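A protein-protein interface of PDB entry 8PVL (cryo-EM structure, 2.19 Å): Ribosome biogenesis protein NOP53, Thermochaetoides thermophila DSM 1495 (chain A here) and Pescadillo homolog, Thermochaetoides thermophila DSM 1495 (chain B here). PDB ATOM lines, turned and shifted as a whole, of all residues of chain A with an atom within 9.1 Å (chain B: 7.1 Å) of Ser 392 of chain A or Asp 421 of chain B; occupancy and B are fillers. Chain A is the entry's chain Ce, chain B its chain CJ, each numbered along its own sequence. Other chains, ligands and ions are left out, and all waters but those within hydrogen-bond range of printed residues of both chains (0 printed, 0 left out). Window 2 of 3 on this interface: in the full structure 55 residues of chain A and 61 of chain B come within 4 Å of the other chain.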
ATOM      1  N   TYR A 215     -17.229  18.701   0.385  1.00  0.00           N
ATOM      2  CA  TYR A 215     -18.369  18.513  -0.505  1.00  0.00           C
ATOM      3  C   TYR A 215     -19.518  17.804   0.201  1.00  0.00           C
ATOM      4  O   TYR A 215     -20.681  17.972  -0.183  1.00  0.00           O
ATOM      5  CB  TYR A 215     -17.935  17.743  -1.754  1.00  0.00           C
ATOM      6  CG  TYR A 215     -18.147  16.246  -1.680  1.00  0.00           C
ATOM      7  CD1 TYR A 215     -17.326  15.446  -0.895  1.00  0.00           C
ATOM      8  CD2 TYR A 215     -19.162  15.633  -2.402  1.00  0.00           C
ATOM      9  CE1 TYR A 215     -17.517  14.083  -0.827  1.00  0.00           C
ATOM     10  CE2 TYR A 215     -19.360  14.272  -2.340  1.00  0.00           C
ATOM     11  CZ  TYR A 215     -18.533  13.502  -1.552  1.00  0.00           C
ATOM     12  OH  TYR A 215     -18.727  12.144  -1.487  1.00  0.00           O
ATOM     13  N   ASN A 216     -19.213  17.016   1.226  1.00  0.00           N
ATOM     14  CA  ASN A 216     -20.210  16.327   2.044  1.00  0.00           C
ATOM     15  C   ASN A 216     -19.853  16.575   3.503  1.00  0.00           C
ATOM     16  O   ASN A 216     -19.385  15.675   4.207  1.00  0.00           O
ATOM     17  CB  ASN A 216     -20.247  14.835   1.713  1.00  0.00           C
ATOM     18  CG  ASN A 216     -21.368  14.106   2.415  1.00  0.00           C
ATOM     19  OD1 ASN A 216     -22.335  14.715   2.866  1.00  0.00           O
ATOM     20  ND2 ASN A 216     -21.247  12.788   2.506  1.00  0.00           N
ATOM     21  N   GLU A 388     -29.426  23.958  -2.327  1.00  0.00           N
ATOM     22  CA  GLU A 388     -28.591  23.413  -3.387  1.00  0.00           C
ATOM     23  C   GLU A 388     -27.777  22.203  -2.948  1.00  0.00           C
ATOM     24  O   GLU A 388     -26.917  21.749  -3.709  1.00  0.00           O
ATOM     25  CB  GLU A 388     -27.644  24.490  -3.923  1.00  0.00           C
ATOM     26  CG  GLU A 388     -28.229  25.887  -3.955  1.00  0.00           C
ATOM     27  CD  GLU A 388     -27.161  26.961  -3.990  1.00  0.00           C
ATOM     28  OE1 GLU A 388     -25.990  26.646  -3.687  1.00  0.00           O
ATOM     29  OE2 GLU A 388     -27.490  28.119  -4.323  1.00  0.00           O
ATOM     30  N   LEU A 389     -28.010  21.686  -1.744  1.00  0.00           N
ATOM     31  CA  LEU A 389     -27.223  20.568  -1.241  1.00  0.00           C
ATOM     32  C   LEU A 389     -27.538  19.292  -2.010  1.00  0.00           C
ATOM     33  O   LEU A 389     -28.698  18.989  -2.298  1.00  0.00           O
ATOM     34  CB  LEU A 389     -27.488  20.361   0.249  1.00  0.00           C
ATOM     35  CG  LEU A 389     -26.682  21.237   1.210  1.00  0.00           C
ATOM     36  CD1 LEU A 389     -27.141  21.023   2.642  1.00  0.00           C
ATOM     37  CD2 LEU A 389     -25.197  20.954   1.073  1.00  0.00           C
ATOM     38  N   GLU A 390     -26.491  18.542  -2.340  1.00  0.00           N
ATOM     39  CA  GLU A 390     -26.614  17.302  -3.088  1.00  0.00           C
ATOM     40  C   GLU A 390     -25.994  16.157  -2.299  1.00  0.00           C
ATOM     41  O   GLU A 390     -25.213  16.366  -1.367  1.00  0.00           O
ATOM     42  CB  GLU A 390     -25.950  17.414  -4.467  1.00  0.00           C
ATOM     43  CG  GLU A 390     -26.486  18.546  -5.328  1.00  0.00           C
ATOM     44  CD  GLU A 390     -27.835  18.232  -5.949  1.00  0.00           C
ATOM     45  OE1 GLU A 390     -28.243  17.052  -5.938  1.00  0.00           O
ATOM     46  OE2 GLU A 390     -28.488  19.168  -6.454  1.00  0.00           O
ATOM     47  N   ASP A 391     -26.354  14.935  -2.687  1.00  0.00           N
ATOM     48  CA  ASP A 391     -25.947  13.734  -1.973  1.00  0.00           C
ATOM     49  C   ASP A 391     -24.944  12.891  -2.748  1.00  0.00           C
ATOM     50  O   ASP A 391     -24.731  11.725  -2.401  1.00  0.00           O
ATOM     51  CB  ASP A 391     -27.177  12.892  -1.627  1.00  0.00           C
ATOM     52  CG  ASP A 391     -28.179  12.836  -2.763  1.00  0.00           C
ATOM     53  OD1 ASP A 391     -27.852  13.308  -3.872  1.00  0.00           O
ATOM     54  OD2 ASP A 391     -29.296  12.319  -2.547  1.00  0.00           O
ATOM     55  N   SER A 392     -24.321  13.445  -3.785  1.00  0.00           N
ATOM     56  CA  SER A 392     -23.393  12.687  -4.610  1.00  0.00           C
ATOM     57  C   SER A 392     -22.284  13.600  -5.109  1.00  0.00           C
ATOM     58  O   SER A 392     -22.445  14.818  -5.206  1.00  0.00           O
ATOM     59  CB  SER A 392     -24.106  12.033  -5.799  1.00  0.00           C
ATOM     60  OG  SER A 392     -24.502  13.006  -6.748  1.00  0.00           O
ATOM     61  N   LEU A 393     -21.140  12.986  -5.419  1.00  0.00           N
ATOM     62  CA  LEU A 393     -20.037  13.727  -6.020  1.00  0.00           C
ATOM     63  C   LEU A 393     -20.339  14.105  -7.465  1.00  0.00           C
ATOM     64  O   LEU A 393     -19.845  15.127  -7.952  1.00  0.00           O
ATOM     65  CB  LEU A 393     -18.751  12.903  -5.941  1.00  0.00           C
ATOM     66  CG  LEU A 393     -17.447  13.564  -6.390  1.00  0.00           C
ATOM     67  CD1 LEU A 393     -17.126  14.771  -5.528  1.00  0.00           C
ATOM     68  CD2 LEU A 393     -16.305  12.566  -6.374  1.00  0.00           C
ATOM     69  N   ARG A 394     -21.144  13.293  -8.158  1.00  0.00           N
ATOM     70  CA  ARG A 394     -21.467  13.561  -9.557  1.00  0.00           C
ATOM     71  C   ARG A 394     -22.268  14.846  -9.712  1.00  0.00           C
ATOM     72  O   ARG A 394     -22.036  15.625 -10.642  1.00  0.00           O
ATOM     73  CB  ARG A 394     -22.237  12.381 -10.148  1.00  0.00           C
ATOM     74  CG  ARG A 394     -22.630  12.554 -11.604  1.00  0.00           C
ATOM     75  CD  ARG A 394     -23.495  11.404 -12.075  1.00  0.00           C
ATOM     76  NE  ARG A 394     -24.571  11.121 -11.133  1.00  0.00           N
ATOM     77  CZ  ARG A 394     -25.737  11.751 -11.116  1.00  0.00           C
ATOM     78  NH1 ARG A 394     -26.018  12.707 -11.986  1.00  0.00           N
ATOM     79  NH2 ARG A 394     -26.643  11.417 -10.202  1.00  0.00           N
ATOM     80  N   ARG A 395     -23.206  15.093  -8.803  1.00  0.00           N
ATOM     81  CA  ARG A 395     -24.066  16.263  -8.876  1.00  0.00           C
ATOM     82  C   ARG A 395     -23.497  17.462  -8.131  1.00  0.00           C
ATOM     83  O   ARG A 395     -24.223  18.432  -7.900  1.00  0.00           O
ATOM     84  CB  ARG A 395     -25.457  15.928  -8.339  1.00  0.00           C
ATOM     85  CG  ARG A 395     -26.466  15.632  -9.429  1.00  0.00           C
ATOM     86  CD  ARG A 395     -27.876  15.519  -8.876  1.00  0.00           C
ATOM     87  NE  ARG A 395     -28.553  16.810  -8.825  1.00  0.00           N
ATOM     88  CZ  ARG A 395     -29.022  17.465  -9.879  1.00  0.00           C
ATOM     89  NH1 ARG A 395     -28.954  16.958 -11.100  1.00  0.00           N
ATOM     90  NH2 ARG A 395     -29.583  18.658  -9.703  1.00  0.00           N
ATOM     91  N   LEU A 396     -22.225  17.415  -7.749  1.00  0.00           N
ATOM     92  CA  LEU A 396     -21.607  18.534  -7.054  1.00  0.00           C
ATOM     93  C   LEU A 396     -21.395  19.701  -8.009  1.00  0.00           C
ATOM     94  O   LEU A 396     -20.872  19.529  -9.114  1.00  0.00           O
ATOM     95  CB  LEU A 396     -20.278  18.103  -6.439  1.00  0.00           C
ATOM     96  CG  LEU A 396     -19.294  19.203  -6.036  1.00  0.00           C
ATOM     97  CD1 LEU A 396     -19.805  19.972  -4.831  1.00  0.00           C
ATOM     98  CD2 LEU A 396     -17.937  18.604  -5.744  1.00  0.00           C
ATOM     99  N   LYS A 397     -21.808  20.891  -7.578  1.00  0.00           N
ATOM    100  CA  LYS A 397     -21.588  22.120  -8.324  1.00  0.00           C
ATOM    101  C   LYS A 397     -20.400  22.835  -7.696  1.00  0.00           C
ATOM    102  O   LYS A 397     -20.533  23.393  -6.597  1.00  0.00           O
ATOM    103  CB  LYS A 397     -22.839  22.999  -8.282  1.00  0.00           C
ATOM    104  CG  LYS A 397     -22.684  24.376  -8.899  1.00  0.00           C
ATOM    105  CD  LYS A 397     -23.206  24.409 -10.323  1.00  0.00           C
ATOM    106  CE  LYS A 397     -24.613  23.834 -10.428  1.00  0.00           C
ATOM    107  NZ  LYS A 397     -25.599  24.601  -9.621  1.00  0.00           N
ATOM    108  N   SER B 375     -16.482   3.188 -13.042  1.00  0.00           N
ATOM    109  CA  SER B 375     -17.571   3.385 -13.982  1.00  0.00           C
ATOM    110  C   SER B 375     -17.360   4.676 -14.768  1.00  0.00           C
ATOM    111  O   SER B 375     -16.408   5.429 -14.546  1.00  0.00           O
ATOM    112  CB  SER B 375     -18.910   3.391 -13.253  1.00  0.00           C
ATOM    113  OG  SER B 375     -19.207   2.102 -12.749  1.00  0.00           O
ATOM    114  N   GLU B 377     -19.179   7.419 -14.826  1.00  0.00           N
ATOM    115  CA  GLU B 377     -19.522   8.644 -14.119  1.00  0.00           C
ATOM    116  C   GLU B 377     -18.561   8.977 -12.983  1.00  0.00           C
ATOM    117  O   GLU B 377     -18.776   9.978 -12.291  1.00  0.00           O
ATOM    118  CB  GLU B 377     -20.947   8.535 -13.573  1.00  0.00           C
ATOM    119  CG  GLU B 377     -21.121   7.460 -12.509  1.00  0.00           C
ATOM    120  CD  GLU B 377     -21.450   6.093 -13.079  1.00  0.00           C
ATOM    121  OE1 GLU B 377     -21.352   5.914 -14.311  1.00  0.00           O
ATOM    122  OE2 GLU B 377     -21.799   5.190 -12.293  1.00  0.00           O
ATOM    123  N   THR B 378     -17.509   8.166 -12.771  1.00  0.00           N
ATOM    124  CA  THR B 378     -16.551   8.335 -11.686  1.00  0.00           C
ATOM    125  C   THR B 378     -15.309   9.085 -12.166  1.00  0.00           C
ATOM    126  O   THR B 378     -14.888   8.929 -13.317  1.00  0.00           O
ATOM    127  CB  THR B 378     -16.147   6.975 -11.126  1.00  0.00           C
ATOM    128  OG1 THR B 378     -15.499   6.208 -12.147  1.00  0.00           O
ATOM    129  CG2 THR B 378     -17.369   6.225 -10.626  1.00  0.00           C
ATOM    130  N   PRO B 379     -14.689   9.915 -11.304  1.00  0.00           N
ATOM    131  CA  PRO B 379     -13.536  10.721 -11.734  1.00  0.00           C
ATOM    132  C   PRO B 379     -12.268   9.890 -11.872  1.00  0.00           C
ATOM    133  O   PRO B 379     -11.602   9.554 -10.883  1.00  0.00           O
ATOM    134  CB  PRO B 379     -13.421  11.778 -10.625  1.00  0.00           C
ATOM    135  CG  PRO B 379     -14.090  11.198  -9.450  1.00  0.00           C
ATOM    136  CD  PRO B 379     -15.134  10.252  -9.940  1.00  0.00           C
ATOM    137  N   ILE B 419     -16.424   1.103  -8.509  1.00  0.00           N
ATOM    138  CA  ILE B 419     -16.760   2.458  -8.089  1.00  0.00           C
ATOM    139  C   ILE B 419     -17.890   2.968  -8.969  1.00  0.00           C
ATOM    140  O   ILE B 419     -17.791   2.943 -10.201  1.00  0.00           O
ATOM    141  CB  ILE B 419     -15.535   3.381  -8.170  1.00  0.00           C
ATOM    142  CG1 ILE B 419     -14.303   2.690  -7.583  1.00  0.00           C
ATOM    143  CG2 ILE B 419     -15.806   4.694  -7.453  1.00  0.00           C
ATOM    144  CD1 ILE B 419     -14.389   2.429  -6.101  1.00  0.00           C
ATOM    145  N   ILE B 420     -18.968   3.426  -8.338  1.00  0.00           N
ATOM    146  CA  ILE B 420     -20.163   3.876  -9.037  1.00  0.00           C
ATOM    147  C   ILE B 420     -20.645   5.188  -8.432  1.00  0.00           C
ATOM    148  O   ILE B 420     -20.445   5.458  -7.244  1.00  0.00           O
ATOM    149  CB  ILE B 420     -21.275   2.793  -9.007  1.00  0.00           C
ATOM    150  CG1 ILE B 420     -21.498   2.258  -7.586  1.00  0.00           C
ATOM    151  CG2 ILE B 420     -20.971   1.665  -9.980  1.00  0.00           C
ATOM    152  CD1 ILE B 420     -22.572   2.954  -6.788  1.00  0.00           C
ATOM    153  N   ASP B 421     -21.277   6.015  -9.268  1.00  0.00           N
ATOM    154  CA  ASP B 421     -21.902   7.250  -8.808  1.00  0.00           C
ATOM    155  C   ASP B 421     -23.226   7.496  -9.523  1.00  0.00           C
ATOM    156  O   ASP B 421     -23.606   8.648  -9.755  1.00  0.00           O
ATOM    157  CB  ASP B 421     -20.966   8.447  -8.998  1.00  0.00           C
ATOM    158  CG  ASP B 421     -21.142   9.501  -7.923  1.00  0.00           C
ATOM    159  OD1 ASP B 421     -22.088   9.379  -7.118  1.00  0.00           O
ATOM    160  OD2 ASP B 421     -20.335  10.453  -7.882  1.00  0.00           O
ATOM    161  N   ARG B 422     -23.939   6.427  -9.879  1.00  0.00           N
ATOM    162  CA  ARG B 422     -25.175   6.506 -10.637  1.00  0.00           C
ATOM    163  C   ARG B 422     -26.347   5.983  -9.814  1.00  0.00           C
ATOM    164  O   ARG B 422     -26.209   4.969  -9.120  1.00  0.00           O
ATOM    165  CB  ARG B 422     -25.065   5.693 -11.935  1.00  0.00           C
ATOM    166  CG  ARG B 422     -25.906   6.221 -13.083  1.00  0.00           C
ATOM    167  CD  ARG B 422     -25.851   5.297 -14.289  1.00  0.00           C
ATOM    168  NE  ARG B 422     -24.539   5.298 -14.923  1.00  0.00           N
ATOM    169  CZ  ARG B 422     -24.110   6.228 -15.766  1.00  0.00           C
ATOM    170  NH1 ARG B 422     -24.869   7.255 -16.110  1.00  0.00           N
ATOM    171  NH2 ARG B 422     -22.886   6.125 -16.277  1.00  0.00           N
ATOM    172  N   PRO B 423     -27.511   6.651  -9.860  1.00  0.00           N
ATOM    173  CA  PRO B 423     -28.704   6.163  -9.160  1.00  0.00           C
ATOM    174  C   PRO B 423     -29.277   4.898  -9.792  1.00  0.00           C
ATOM    175  O   PRO B 423     -29.538   3.937  -9.070  1.00  0.00           O
ATOM    176  CB  PRO B 423     -29.690   7.327  -9.291  1.00  0.00           C
ATOM    177  CG  PRO B 423     -29.225   8.087 -10.482  1.00  0.00           C
ATOM    178  CD  PRO B 423     -27.736   7.972 -10.471  1.00  0.00           C
ATOM    179  N   VAL B 456     -19.169   0.498  -4.466  1.00  0.00           N
ATOM    180  CA  VAL B 456     -18.981   1.618  -3.557  1.00  0.00           C
ATOM    181  C   VAL B 456     -19.011   2.930  -4.326  1.00  0.00           C
ATOM    182  O   VAL B 456     -18.800   2.977  -5.538  1.00  0.00           O
ATOM    183  CB  VAL B 456     -17.668   1.503  -2.752  1.00  0.00           C
ATOM    184  CG1 VAL B 456     -17.913   0.771  -1.446  1.00  0.00           C
ATOM    185  CG2 VAL B 456     -16.608   0.793  -3.568  1.00  0.00           C
ATOM    186  N   GLN B 457     -19.293   4.001  -3.593  1.00  0.00           N
ATOM    187  CA  GLN B 457     -19.200   5.356  -4.103  1.00  0.00           C
ATOM    188  C   GLN B 457     -17.761   5.854  -3.978  1.00  0.00           C
ATOM    189  O   GLN B 457     -16.970   5.285  -3.223  1.00  0.00           O
ATOM    190  CB  GLN B 457     -20.171   6.257  -3.345  1.00  0.00           C
ATOM    191  CG  GLN B 457     -21.609   5.775  -3.407  1.00  0.00           C
ATOM    192  CD  GLN B 457     -22.611   6.865  -3.095  1.00  0.00           C
ATOM    193  OE1 GLN B 457     -22.422   8.023  -3.467  1.00  0.00           O
ATOM    194  NE2 GLN B 457     -23.687   6.501  -2.411  1.00  0.00           N
ATOM    195  N   PRO B 458     -17.383   6.891  -4.741  1.00  0.00           N
ATOM    196  CA  PRO B 458     -15.985   7.362  -4.706  1.00  0.00           C
ATOM    197  C   PRO B 458     -15.492   7.839  -3.345  1.00  0.00           C
ATOM    198  O   PRO B 458     -14.280   7.785  -3.106  1.00  0.00           O
ATOM    199  CB  PRO B 458     -15.969   8.510  -5.728  1.00  0.00           C
ATOM    200  CG  PRO B 458     -17.365   8.636  -6.252  1.00  0.00           C
ATOM    201  CD  PRO B 458     -18.067   7.367  -5.954  1.00  0.00           C
ATOM    202  N   GLN B 459     -16.375   8.288  -2.445  1.00  0.00           N
ATOM    203  CA  GLN B 459     -15.936   8.749  -1.128  1.00  0.00           C
ATOM    204  C   GLN B 459     -15.339   7.626  -0.283  1.00  0.00           C
ATOM    205  O   GLN B 459     -14.578   7.907   0.652  1.00  0.00           O
ATOM    206  CB  GLN B 459     -17.107   9.401  -0.385  1.00  0.00           C
ATOM    207  CG  GLN B 459     -16.705  10.243   0.822  1.00  0.00           C
ATOM    208  CD  GLN B 459     -17.885  10.891   1.508  1.00  0.00           C
ATOM    209  OE1 GLN B 459     -18.759  11.460   0.859  1.00  0.00           O
ATOM    210  NE2 GLN B 459     -17.917  10.805   2.831  1.00  0.00           N
ATOM    211  N   LEU B 482     -24.312   9.038   2.329  1.00  0.00           N
ATOM    212  CA  LEU B 482     -22.908   8.864   2.656  1.00  0.00           C
ATOM    213  C   LEU B 482     -22.589   9.461   4.026  1.00  0.00           C
ATOM    214  O   LEU B 482     -23.245  10.408   4.468  1.00  0.00           O
ATOM    215  CB  LEU B 482     -22.033   9.520   1.591  1.00  0.00           C
ATOM    216  CG  LEU B 482     -21.961   8.818   0.235  1.00  0.00           C
ATOM    217  CD1 LEU B 482     -21.009   9.546  -0.696  1.00  0.00           C
ATOM    218  CD2 LEU B 482     -21.546   7.370   0.403  1.00  0.00           C
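The side-chain amide oxygen of Gln 459 of chain B lies within hydrogen-bond range of the side-chain hydroxyl of Tyr 215 of chain A (2.4 Å).
The side-chain amide oxygen (OE1) of Gln 459 of chain B is in hydrogen-bond range of the side-chain amide nitrogen (ND2) of Asn 216 of chain A.
N of Arg 394 of chain A sits at hydrogen-bond distance from OD2 of Asp 421 of chain B, 3.0 Å away.
The side-chain hydroxyl of Ser 392 of chain A is in hydrogen-bond range of the backbone NH of Arg 395 of chain A (3.2 Å).
The backbone NH of Asp 421 of chain B lies within hydrogen-bond range of the side-chain carboxylate of Glu 377 of chain B (3.2 Å).
Among the printed residues, merely in contact across the chains: Tyr 215 of chain A with Leu 482 of chain B (3.5 Å), Asn 216 of chain A with Leu 482 of chain B (3.5 Å), Ser 392 of chain A with Asp 421 of chain B (3.6 Å), Leu 393 of chain A with Asp 421 of chain B (3.5 Å) and Arg 394 of chain A with Pro 423 of chain B (3.6 Å).
Of the printed residues of chain B, Tyr 215 of chain A touches Gln 459 (2.4 Å) and Leu 482 (3.5 Å).
Glu 390 of chain A touches none of the printed residues of chain B.
Ser 392 of chain A touches just one residue of chain B: Asp 421 (3.6 Å).
Printed residues of chain B within 4 Å of Arg 394 of chain A: Asp 421 and Pro 423.
No residue of chain A comes within 4 Å of Ile 420 of chain B.
Asp 421 of chain B touches just these residues of chain A: Ser 392 (3.6 Å), Leu 393 (3.5 Å) and Arg 394 (3.0 Å).
The nearest printed residue of chain A that does not touch Pro 423 of chain B is Ser 392 of chain A (7.0 Å).
Of the 14 printed residues of chain B, 4 touch a printed residue of chain A.
Among the printed residues, 8 pairs touch across the chains.
Among the printed residues, no Asp or Glu carboxylate lies within 4 Å of a Lys or Arg side-chain nitrogen of the other chain.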
